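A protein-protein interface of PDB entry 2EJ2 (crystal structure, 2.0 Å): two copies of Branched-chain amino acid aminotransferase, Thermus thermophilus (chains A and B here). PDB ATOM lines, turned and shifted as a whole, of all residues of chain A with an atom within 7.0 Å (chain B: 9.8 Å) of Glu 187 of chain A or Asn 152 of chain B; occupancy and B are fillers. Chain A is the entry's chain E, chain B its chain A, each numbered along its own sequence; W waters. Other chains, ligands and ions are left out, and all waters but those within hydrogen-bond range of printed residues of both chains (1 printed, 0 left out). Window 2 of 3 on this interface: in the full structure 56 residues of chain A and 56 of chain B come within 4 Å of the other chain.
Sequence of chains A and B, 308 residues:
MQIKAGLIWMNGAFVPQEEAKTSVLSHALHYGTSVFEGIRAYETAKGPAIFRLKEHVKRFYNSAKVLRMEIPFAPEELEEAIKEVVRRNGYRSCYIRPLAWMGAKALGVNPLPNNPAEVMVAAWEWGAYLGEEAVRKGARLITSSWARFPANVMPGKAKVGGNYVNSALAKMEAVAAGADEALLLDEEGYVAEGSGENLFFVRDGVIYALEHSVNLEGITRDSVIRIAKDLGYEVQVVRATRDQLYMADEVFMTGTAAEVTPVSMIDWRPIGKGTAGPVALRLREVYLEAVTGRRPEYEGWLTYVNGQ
Of chain B, only Asn 152 (2.8 Å) and Val 153 (3.7 Å) come within 4 Å of Ala 147 of chain A. Of the printed residues of chain B, Phe 149 of chain A touches Val 153. Of the printed residues of chain B, Asn 166 of chain A touches Val 153. No residue of chain B comes within 4 Å of Asp 186 of chain A. Glu 187 of chain A touches three residues of chain B. No residue of chain B comes within 4 Å of Glu 188 of chain A. Printed residues of chain A within 4 Å of Pro 150 of chain B: Glu 187 (3.2 Å). Asn 152 of chain B touches just these residues of chain A: Trp 146 (3.4 Å), Ala 147 (2.8 Å) and Glu 187 (2.6 Å). Printed residues of chain A within 4 Å of Val 153 of chain B: Trp 146, Ala 147, Phe 149, Asn 166 and Glu 187. Asn 163 of chain B touches none of the printed residues of chain A. The nearest printed residue of chain B that does not touch Glu 187 of chain A is Glu 187 of chain B (5.6 Å).
Among the printed residues, pairs that only touch across the chains: Trp 146 of chain A with Asn 152 of chain B (3.4 Å), Trp 146 of chain A with Val 153 of chain B (3.8 Å), Ala 147 of chain A with Val 153 of chain B (3.7 Å), Phe 149 of chain A with Val 153 of chain B (3.5 Å), Pro 150 of chain A with Glu 187 of chain B (3.1 Å), Glu 187 of chain A with Pro 150 of chain B (3.2 Å) and Glu 187 of chain A with Val 153 of chain B (3.5 Å).
The backbone NH of Ala 147 of chain A is in hydrogen-bond range of the backbone carbonyl oxygen of Asn 152 of chain B. The side-chain amide oxygen (OD1) of Asn 152 of chain B sits close to the side-chain carboxylate (OE2) of Glu 187 of chain A. O of Val 153 of chain B sits at hydrogen-bond distance from ND2 of Asn 166 of chain A (2.8 Å).
Hydrophobic or aromatic side chains of chain A within 4 Å of the printed part of chain B: Trp 146, Ala 147, Phe 149 and Pro 150. Printed residues of chain B that touch a printed residue of chain A: Pro 150, Asn 152, Val 153 and Glu 187. Hydrophobic or aromatic side chains of chain B that line the printed part of chain A: Pro 150 and Val 153. Along chain B the printed residues that touch a printed residue of chain A span positions 150 to 187.
Water W1 lies within hydrogen-bond range of O of Ser 145 of chain A (2.7 Å) and ND2 of Asn 152 of chain B (3.0 Å).
The backbone carbonyl oxygen (O) of Ala 147 of chain A is in hydrogen-bond range of the side-chain amide nitrogen (ND2) of Asn 166 of chain A (3.1 Å). NH1 of Arg 148 of chain A is in hydrogen-bond range of OD1 of Asn 166 of chain A (3.0 Å).
Pro 150 of chain A touches Glu 187 of chain B, and with the chains exchanged Glu 187 of chain A touches Pro 150 of chain B. Of the 10 pairs that touch across the chains among the printed residues, 2 have their exchanged pair printed and touching as well.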
ATOM      1  N   SER A 145      19.684  -6.405 -13.359  1.00  0.00           N
ATOM      2  CA  SER A 145      19.523  -6.229 -11.916  1.00  0.00           C
ATOM      3  C   SER A 145      20.846  -5.677 -11.378  1.00  0.00           C
ATOM      4  O   SER A 145      21.032  -5.521 -10.169  1.00  0.00           O
ATOM      5  CB  SER A 145      19.192  -7.560 -11.234  1.00  0.00           C
ATOM      6  OG  SER A 145      20.241  -8.495 -11.414  1.00  0.00           O
ATOM      7  N   TRP A 146      21.774  -5.412 -12.294  1.00  0.00           N
ATOM      8  CA  TRP A 146      23.065  -4.827 -11.943  1.00  0.00           C
ATOM      9  C   TRP A 146      23.002  -3.389 -12.429  1.00  0.00           C
ATOM     10  O   TRP A 146      22.755  -3.141 -13.605  1.00  0.00           O
ATOM     11  CB  TRP A 146      24.226  -5.554 -12.635  1.00  0.00           C
ATOM     12  CG  TRP A 146      24.461  -6.926 -12.092  1.00  0.00           C
ATOM     13  CD1 TRP A 146      23.912  -8.091 -12.540  1.00  0.00           C
ATOM     14  CD2 TRP A 146      25.228  -7.263 -10.930  1.00  0.00           C
ATOM     15  NE1 TRP A 146      24.282  -9.133 -11.726  1.00  0.00           N
ATOM     16  CE2 TRP A 146      25.090  -8.653 -10.728  1.00  0.00           C
ATOM     17  CE3 TRP A 146      26.016  -6.523 -10.038  1.00  0.00           C
ATOM     18  CZ2 TRP A 146      25.711  -9.324  -9.666  1.00  0.00           C
ATOM     19  CZ3 TRP A 146      26.634  -7.188  -8.982  1.00  0.00           C
ATOM     20  CH2 TRP A 146      26.476  -8.577  -8.806  1.00  0.00           C
ATOM     21  N   ALA A 147      23.207  -2.443 -11.518  1.00  0.00           N
ATOM     22  CA  ALA A 147      23.155  -1.034 -11.866  1.00  0.00           C
ATOM     23  C   ALA A 147      24.496  -0.562 -12.409  1.00  0.00           C
ATOM     24  O   ALA A 147      25.549  -1.034 -11.981  1.00  0.00           O
ATOM     25  CB  ALA A 147      22.771  -0.211 -10.648  1.00  0.00           C
ATOM     26  N   ARG A 148      24.452   0.359 -13.362  1.00  0.00           N
ATOM     27  CA  ARG A 148      25.673   0.898 -13.932  1.00  0.00           C
ATOM     28  C   ARG A 148      26.366   1.664 -12.805  1.00  0.00           C
ATOM     29  O   ARG A 148      25.710   2.337 -12.008  1.00  0.00           O
ATOM     30  CB  ARG A 148      25.340   1.834 -15.093  1.00  0.00           C
ATOM     31  CG  ARG A 148      26.502   2.069 -16.025  1.00  0.00           C
ATOM     32  CD  ARG A 148      27.002   0.740 -16.572  1.00  0.00           C
ATOM     33  NE  ARG A 148      28.078   0.933 -17.532  1.00  0.00           N
ATOM     34  CZ  ARG A 148      28.911  -0.023 -17.936  1.00  0.00           C
ATOM     35  NH1 ARG A 148      28.807  -1.265 -17.465  1.00  0.00           N
ATOM     36  NH2 ARG A 148      29.859   0.275 -18.811  1.00  0.00           N
ATOM     37  N   PHE A 149      27.685   1.555 -12.729  1.00  0.00           N
ATOM     38  CA  PHE A 149      28.431   2.220 -11.668  1.00  0.00           C
ATOM     39  C   PHE A 149      28.349   3.744 -11.597  1.00  0.00           C
ATOM     40  O   PHE A 149      28.432   4.434 -12.610  1.00  0.00           O
ATOM     41  CB  PHE A 149      29.909   1.803 -11.731  1.00  0.00           C
ATOM     42  CG  PHE A 149      30.420   1.569 -13.130  1.00  0.00           C
ATOM     43  CD1 PHE A 149      30.399   2.587 -14.077  1.00  0.00           C
ATOM     44  CD2 PHE A 149      30.921   0.325 -13.498  1.00  0.00           C
ATOM     45  CE1 PHE A 149      30.871   2.366 -15.374  1.00  0.00           C
ATOM     46  CE2 PHE A 149      31.394   0.094 -14.788  1.00  0.00           C
ATOM     47  CZ  PHE A 149      31.369   1.115 -15.726  1.00  0.00           C
ATOM     48  N   PRO A 150      28.160   4.287 -10.381  1.00  0.00           N
ATOM     49  CA  PRO A 150      28.090   5.740 -10.200  1.00  0.00           C
ATOM     50  C   PRO A 150      29.428   6.330 -10.665  1.00  0.00           C
ATOM     51  O   PRO A 150      30.448   5.636 -10.660  1.00  0.00           O
ATOM     52  CB  PRO A 150      27.896   5.890  -8.694  1.00  0.00           C
ATOM     53  CG  PRO A 150      27.077   4.681  -8.344  1.00  0.00           C
ATOM     54  CD  PRO A 150      27.751   3.581  -9.152  1.00  0.00           C
ATOM     55  N   ASN A 166      31.185  -5.251 -14.488  1.00  0.00           N
ATOM     56  CA  ASN A 166      29.804  -4.794 -14.367  1.00  0.00           C
ATOM     57  C   ASN A 166      29.066  -5.136 -15.673  1.00  0.00           C
ATOM     58  O   ASN A 166      27.945  -5.650 -15.648  1.00  0.00           O
ATOM     59  CB  ASN A 166      29.794  -3.280 -14.083  1.00  0.00           C
ATOM     60  CG  ASN A 166      28.388  -2.717 -13.886  1.00  0.00           C
ATOM     61  OD1 ASN A 166      27.856  -2.031 -14.758  1.00  0.00           O
ATOM     62  ND2 ASN A 166      27.788  -3.000 -12.733  1.00  0.00           N
ATOM     63  N   LEU A 185      20.462   0.188 -15.696  1.00  0.00           N
ATOM     64  CA  LEU A 185      19.964   1.440 -15.144  1.00  0.00           C
ATOM     65  C   LEU A 185      21.071   1.949 -14.228  1.00  0.00           C
ATOM     66  O   LEU A 185      21.926   1.165 -13.803  1.00  0.00           O
ATOM     67  CB  LEU A 185      18.720   1.206 -14.279  1.00  0.00           C
ATOM     68  CG  LEU A 185      17.523   0.466 -14.875  1.00  0.00           C
ATOM     69  CD1 LEU A 185      16.378   0.494 -13.867  1.00  0.00           C
ATOM     70  CD2 LEU A 185      17.104   1.124 -16.180  1.00  0.00           C
ATOM     71  N   ASP A 186      21.072   3.247 -13.935  1.00  0.00           N
ATOM     72  CA  ASP A 186      22.056   3.786 -13.006  1.00  0.00           C
ATOM     73  C   ASP A 186      21.474   3.532 -11.613  1.00  0.00           C
ATOM     74  O   ASP A 186      20.345   3.051 -11.485  1.00  0.00           O
ATOM     75  CB  ASP A 186      22.317   5.289 -13.238  1.00  0.00           C
ATOM     76  CG  ASP A 186      21.059   6.142 -13.147  1.00  0.00           C
ATOM     77  OD1 ASP A 186      20.157   5.825 -12.345  1.00  0.00           O
ATOM     78  OD2 ASP A 186      20.987   7.157 -13.874  1.00  0.00           O
ATOM     79  N   GLU A 187      22.238   3.839 -10.572  1.00  0.00           N
ATOM     80  CA  GLU A 187      21.781   3.593  -9.213  1.00  0.00           C
ATOM     81  C   GLU A 187      20.498   4.350  -8.852  1.00  0.00           C
ATOM     82  O   GLU A 187      19.765   3.941  -7.950  1.00  0.00           O
ATOM     83  CB  GLU A 187      22.903   3.938  -8.229  1.00  0.00           C
ATOM     84  CG  GLU A 187      22.801   3.259  -6.871  1.00  0.00           C
ATOM     85  CD  GLU A 187      22.788   1.737  -6.958  1.00  0.00           C
ATOM     86  OE1 GLU A 187      21.703   1.168  -7.180  1.00  0.00           O
ATOM     87  OE2 GLU A 187      23.860   1.104  -6.810  1.00  0.00           O
ATOM     88  N   GLU A 188      20.221   5.440  -9.565  1.00  0.00           N
ATOM     89  CA  GLU A 188      19.029   6.239  -9.296  1.00  0.00           C
ATOM     90  C   GLU A 188      17.768   5.671  -9.946  1.00  0.00           C
ATOM     91  O   GLU A 188      16.659   6.099  -9.627  1.00  0.00           O
ATOM     92  CB  GLU A 188      19.239   7.688  -9.752  1.00  0.00           C
ATOM     93  CG  GLU A 188      20.187   8.494  -8.858  1.00  0.00           C
ATOM     94  CD  GLU A 188      21.611   7.971  -8.876  1.00  0.00           C
ATOM     95  OE1 GLU A 188      22.158   7.775  -9.983  1.00  0.00           O
ATOM     96  OE2 GLU A 188      22.189   7.761  -7.786  1.00  0.00           O
ATOM     97  N   GLY A 189      17.942   4.716 -10.854  1.00  0.00           N
ATOM     98  CA  GLY A 189      16.800   4.104 -11.511  1.00  0.00           C
ATOM     99  C   GLY A 189      16.566   4.528 -12.951  1.00  0.00           C
ATOM    100  O   GLY A 189      15.640   4.040 -13.592  1.00  0.00           O
ATOM    101  N   TYR A 190      17.382   5.441 -13.467  1.00  0.00           N
ATOM    102  CA  TYR A 190      17.218   5.884 -14.850  1.00  0.00           C
ATOM    103  C   TYR A 190      17.997   4.978 -15.787  1.00  0.00           C
ATOM    104  O   TYR A 190      18.916   4.277 -15.364  1.00  0.00           O
ATOM    105  CB  TYR A 190      17.710   7.324 -15.034  1.00  0.00           C
ATOM    106  CG  TYR A 190      16.871   8.362 -14.323  1.00  0.00           C
ATOM    107  CD1 TYR A 190      17.164   8.748 -13.014  1.00  0.00           C
ATOM    108  CD2 TYR A 190      15.766   8.942 -14.952  1.00  0.00           C
ATOM    109  CE1 TYR A 190      16.378   9.690 -12.350  1.00  0.00           C
ATOM    110  CE2 TYR A 190      14.974   9.879 -14.297  1.00  0.00           C
ATOM    111  CZ  TYR A 190      15.286  10.249 -12.998  1.00  0.00           C
ATOM    112  OH  TYR A 190      14.506  11.183 -12.354  1.00  0.00           O
ATOM    113  N   ALA A 192      20.716   3.865 -18.300  1.00  0.00           N
ATOM    114  CA  ALA A 192      22.099   4.288 -18.469  1.00  0.00           C
ATOM    115  C   ALA A 192      22.549   3.915 -19.876  1.00  0.00           C
ATOM    116  O   ALA A 192      22.508   4.744 -20.781  1.00  0.00           O
ATOM    117  CB  ALA A 192      22.983   3.617 -17.425  1.00  0.00           C
ATOM    118  N   VAL A 214      26.402   8.396 -16.558  1.00  0.00           N
ATOM    119  CA  VAL A 214      27.512   7.543 -16.122  1.00  0.00           C
ATOM    120  C   VAL A 214      28.011   6.622 -17.237  1.00  0.00           C
ATOM    121  O   VAL A 214      28.786   5.690 -16.992  1.00  0.00           O
ATOM    122  CB  VAL A 214      27.087   6.650 -14.938  1.00  0.00           C
ATOM    123  CG1 VAL A 214      26.747   7.506 -13.730  1.00  0.00           C
ATOM    124  CG2 VAL A 214      25.883   5.802 -15.341  1.00  0.00           C
ATOM    125  N   ARG B 148      33.032   3.230  -2.155  1.00  0.00           N
ATOM    126  CA  ARG B 148      33.085   1.791  -2.328  1.00  0.00           C
ATOM    127  C   ARG B 148      31.836   1.441  -3.134  1.00  0.00           C
ATOM    128  O   ARG B 148      30.770   2.017  -2.911  1.00  0.00           O
ATOM    129  CB  ARG B 148      33.057   1.090  -0.969  1.00  0.00           C
ATOM    130  CG  ARG B 148      33.573  -0.332  -1.008  1.00  0.00           C
ATOM    131  CD  ARG B 148      34.967  -0.328  -1.601  1.00  0.00           C
ATOM    132  NE  ARG B 148      35.626  -1.622  -1.532  1.00  0.00           N
ATOM    133  CZ  ARG B 148      36.718  -1.937  -2.225  1.00  0.00           C
ATOM    134  NH1 ARG B 148      37.278  -1.053  -3.047  1.00  0.00           N
ATOM    135  NH2 ARG B 148      37.250  -3.137  -2.094  1.00  0.00           N
ATOM    136  N   PHE B 149      31.968   0.510  -4.074  1.00  0.00           N
ATOM    137  CA  PHE B 149      30.842   0.123  -4.925  1.00  0.00           C
ATOM    138  C   PHE B 149      29.609  -0.444  -4.221  1.00  0.00           C
ATOM    139  O   PHE B 149      29.722  -1.266  -3.317  1.00  0.00           O
ATOM    140  CB  PHE B 149      31.313  -0.882  -5.986  1.00  0.00           C
ATOM    141  CG  PHE B 149      32.463  -1.749  -5.542  1.00  0.00           C
ATOM    142  CD1 PHE B 149      32.326  -2.624  -4.470  1.00  0.00           C
ATOM    143  CD2 PHE B 149      33.691  -1.683  -6.201  1.00  0.00           C
ATOM    144  CE1 PHE B 149      33.396  -3.424  -4.057  1.00  0.00           C
ATOM    145  CE2 PHE B 149      34.767  -2.475  -5.800  1.00  0.00           C
ATOM    146  CZ  PHE B 149      34.619  -3.348  -4.723  1.00  0.00           C
ATOM    147  N   PRO B 150      28.406   0.015  -4.618  1.00  0.00           N
ATOM    148  CA  PRO B 150      27.175  -0.496  -4.000  1.00  0.00           C
ATOM    149  C   PRO B 150      27.111  -1.999  -4.295  1.00  0.00           C
ATOM    150  O   PRO B 150      27.751  -2.476  -5.242  1.00  0.00           O
ATOM    151  CB  PRO B 150      26.076   0.285  -4.718  1.00  0.00           C
ATOM    152  CG  PRO B 150      26.742   1.614  -4.987  1.00  0.00           C
ATOM    153  CD  PRO B 150      28.123   1.185  -5.472  1.00  0.00           C
ATOM    154  N   ALA B 151      26.331  -2.737  -3.506  1.00  0.00           N
ATOM    155  CA  ALA B 151      26.232  -4.187  -3.665  1.00  0.00           C
ATOM    156  C   ALA B 151      25.536  -4.680  -4.933  1.00  0.00           C
ATOM    157  O   ALA B 151      25.475  -5.888  -5.178  1.00  0.00           O
ATOM    158  CB  ALA B 151      25.567  -4.803  -2.423  1.00  0.00           C
ATOM    159  N   ASN B 152      25.004  -3.762  -5.733  1.00  0.00           N
ATOM    160  CA  ASN B 152      24.356  -4.151  -6.981  1.00  0.00           C
ATOM    161  C   ASN B 152      25.124  -3.559  -8.161  1.00  0.00           C
ATOM    162  O   ASN B 152      24.575  -3.400  -9.248  1.00  0.00           O
ATOM    163  CB  ASN B 152      22.894  -3.683  -7.009  1.00  0.00           C
ATOM    164  CG  ASN B 152      22.759  -2.178  -6.953  1.00  0.00           C
ATOM    165  OD1 ASN B 152      23.602  -1.491  -6.376  1.00  0.00           O
ATOM    166  ND2 ASN B 152      21.685  -1.654  -7.540  1.00  0.00           N
ATOM    167  N   VAL B 153      26.395  -3.233  -7.928  1.00  0.00           N
ATOM    168  CA  VAL B 153      27.261  -2.667  -8.962  1.00  0.00           C
ATOM    169  C   VAL B 153      28.477  -3.580  -9.176  1.00  0.00           C
ATOM    170  O   VAL B 153      28.810  -3.943 -10.308  1.00  0.00           O
ATOM    171  CB  VAL B 153      27.724  -1.244  -8.568  1.00  0.00           C
ATOM    172  CG1 VAL B 153      28.736  -0.717  -9.579  1.00  0.00           C
ATOM    173  CG2 VAL B 153      26.515  -0.315  -8.510  1.00  0.00           C
ATOM    174  N   MET B 154      29.138  -3.938  -8.081  1.00  0.00           N
ATOM    175  CA  MET B 154      30.278  -4.849  -8.118  1.00  0.00           C
ATOM    176  C   MET B 154      30.078  -5.781  -6.922  1.00  0.00           C
ATOM    177  O   MET B 154      29.588  -5.354  -5.874  1.00  0.00           O
ATOM    178  CB  MET B 154      31.607  -4.091  -7.976  1.00  0.00           C
ATOM    179  CG  MET B 154      31.895  -3.071  -9.083  1.00  0.00           C
ATOM    180  SD  MET B 154      32.271  -3.791 -10.701  1.00  0.00           S
ATOM    181  CE  MET B 154      34.083  -3.919 -10.614  1.00  0.00           C
ATOM    182  N   PRO B 155      30.439  -7.066  -7.064  1.00  0.00           N
ATOM    183  CA  PRO B 155      30.278  -8.028  -5.966  1.00  0.00           C
ATOM    184  C   PRO B 155      31.357  -7.869  -4.891  1.00  0.00           C
ATOM    185  O   PRO B 155      32.404  -8.534  -4.931  1.00  0.00           O
ATOM    186  CB  PRO B 155      30.354  -9.369  -6.681  1.00  0.00           C
ATOM    187  CG  PRO B 155      31.367  -9.095  -7.756  1.00  0.00           C
ATOM    188  CD  PRO B 155      30.951  -7.730  -8.278  1.00  0.00           C
ATOM    189  N   GLY B 156      31.082  -6.992  -3.930  1.00  0.00           N
ATOM    190  CA  GLY B 156      32.023  -6.708  -2.857  1.00  0.00           C
ATOM    191  C   GLY B 156      32.393  -7.835  -1.909  1.00  0.00           C
ATOM    192  O   GLY B 156      33.363  -7.706  -1.166  1.00  0.00           O
ATOM    193  N   LYS B 157      31.634  -8.929  -1.914  1.00  0.00           N
ATOM    194  CA  LYS B 157      31.930 -10.062  -1.044  1.00  0.00           C
ATOM    195  C   LYS B 157      32.966 -10.982  -1.689  1.00  0.00           C
ATOM    196  O   LYS B 157      33.471 -11.912  -1.061  1.00  0.00           O
ATOM    197  CB  LYS B 157      30.658 -10.868  -0.767  1.00  0.00           C
ATOM    198  CG  LYS B 157      29.569 -10.091  -0.047  1.00  0.00           C
ATOM    199  CD  LYS B 157      29.989  -9.719   1.360  1.00  0.00           C
ATOM    200  CE  LYS B 157      29.143  -8.580   1.905  1.00  0.00           C
ATOM    201  NZ  LYS B 157      29.432  -7.282   1.216  1.00  0.00           N
ATOM    202  N   ASN B 163      37.062  -5.431  -9.329  1.00  0.00           N
ATOM    203  CA  ASN B 163      36.714  -4.699  -8.116  1.00  0.00           C
ATOM    204  C   ASN B 163      37.869  -3.814  -7.667  1.00  0.00           C
ATOM    205  O   ASN B 163      37.659  -2.724  -7.142  1.00  0.00           O
ATOM    206  CB  ASN B 163      36.412  -5.664  -6.965  1.00  0.00           C
ATOM    207  CG  ASN B 163      35.092  -6.390  -7.120  1.00  0.00           C
ATOM    208  OD1 ASN B 163      34.452  -6.344  -8.171  1.00  0.00           O
ATOM    209  ND2 ASN B 163      34.680  -7.080  -6.064  1.00  0.00           N
ATOM    210  N   ASP B 186      30.751   4.374   1.671  1.00  0.00           N
ATOM    211  CA  ASP B 186      29.856   3.800   0.677  1.00  0.00           C
ATOM    212  C   ASP B 186      29.131   5.000   0.055  1.00  0.00           C
ATOM    213  O   ASP B 186      29.296   6.136   0.517  1.00  0.00           O
ATOM    214  CB  ASP B 186      28.862   2.803   1.298  1.00  0.00           C
ATOM    215  CG  ASP B 186      28.046   3.399   2.428  1.00  0.00           C
ATOM    216  OD1 ASP B 186      27.770   4.615   2.402  1.00  0.00           O
ATOM    217  OD2 ASP B 186      27.666   2.634   3.338  1.00  0.00           O
ATOM    218  N   GLU B 187      28.343   4.760  -0.987  1.00  0.00           N
ATOM    219  CA  GLU B 187      27.643   5.837  -1.676  1.00  0.00           C
ATOM    220  C   GLU B 187      26.703   6.635  -0.773  1.00  0.00           C
ATOM    221  O   GLU B 187      26.397   7.790  -1.066  1.00  0.00           O
ATOM    222  CB  GLU B 187      26.872   5.262  -2.870  1.00  0.00           C
ATOM    223  CG  GLU B 187      26.590   6.259  -3.994  1.00  0.00           C
ATOM    224  CD  GLU B 187      27.858   6.868  -4.597  1.00  0.00           C
ATOM    225  OE1 GLU B 187      28.380   7.846  -4.029  1.00  0.00           O
ATOM    226  OE2 GLU B 187      28.335   6.362  -5.637  1.00  0.00           O
ATOM    227  N   GLU B 188      26.255   6.031   0.325  1.00  0.00           N
ATOM    228  CA  GLU B 188      25.355   6.711   1.253  1.00  0.00           C
ATOM    229  C   GLU B 188      26.100   7.612   2.246  1.00  0.00           C
ATOM    230  O   GLU B 188      25.476   8.374   2.989  1.00  0.00           O
ATOM    231  CB  GLU B 188      24.513   5.690   2.026  1.00  0.00           C
ATOM    232  CG  GLU B 188      23.466   4.960   1.190  1.00  0.00           C
ATOM    233  CD  GLU B 188      24.070   4.083   0.103  1.00  0.00           C
ATOM    234  OE1 GLU B 188      24.984   3.290   0.411  1.00  0.00           O
ATOM    235  OE2 GLU B 188      23.623   4.177  -1.057  1.00  0.00           O
ATOM    236  N   SER B 213      28.284  -4.749   5.280  1.00  0.00           N
ATOM    237  CA  SER B 213      27.774  -3.837   4.260  1.00  0.00           C
ATOM    238  C   SER B 213      28.258  -4.231   2.855  1.00  0.00           C
ATOM    239  O   SER B 213      27.984  -5.340   2.395  1.00  0.00           O
ATOM    240  CB  SER B 213      28.152  -2.378   4.583  1.00  0.00           C
ATOM    241  OG  SER B 213      29.543  -2.144   4.481  1.00  0.00           O
ATOM    242  N   VAL B 214      28.977  -3.340   2.180  1.00  0.00           N
ATOM    243  CA  VAL B 214      29.470  -3.629   0.834  1.00  0.00           C
ATOM    244  C   VAL B 214      30.920  -4.116   0.842  1.00  0.00           C
ATOM    245  O   VAL B 214      31.554  -4.218  -0.211  1.00  0.00           O
ATOM    246  CB  VAL B 214      29.394  -2.379  -0.076  1.00  0.00           C
ATOM    247  CG1 VAL B 214      27.941  -1.952  -0.269  1.00  0.00           C
ATOM    248  CG2 VAL B 214      30.205  -1.238   0.534  1.00  0.00           C
HETATM  249  O   HOH W   1      19.770  -3.352  -9.112  1.00  0.00           O
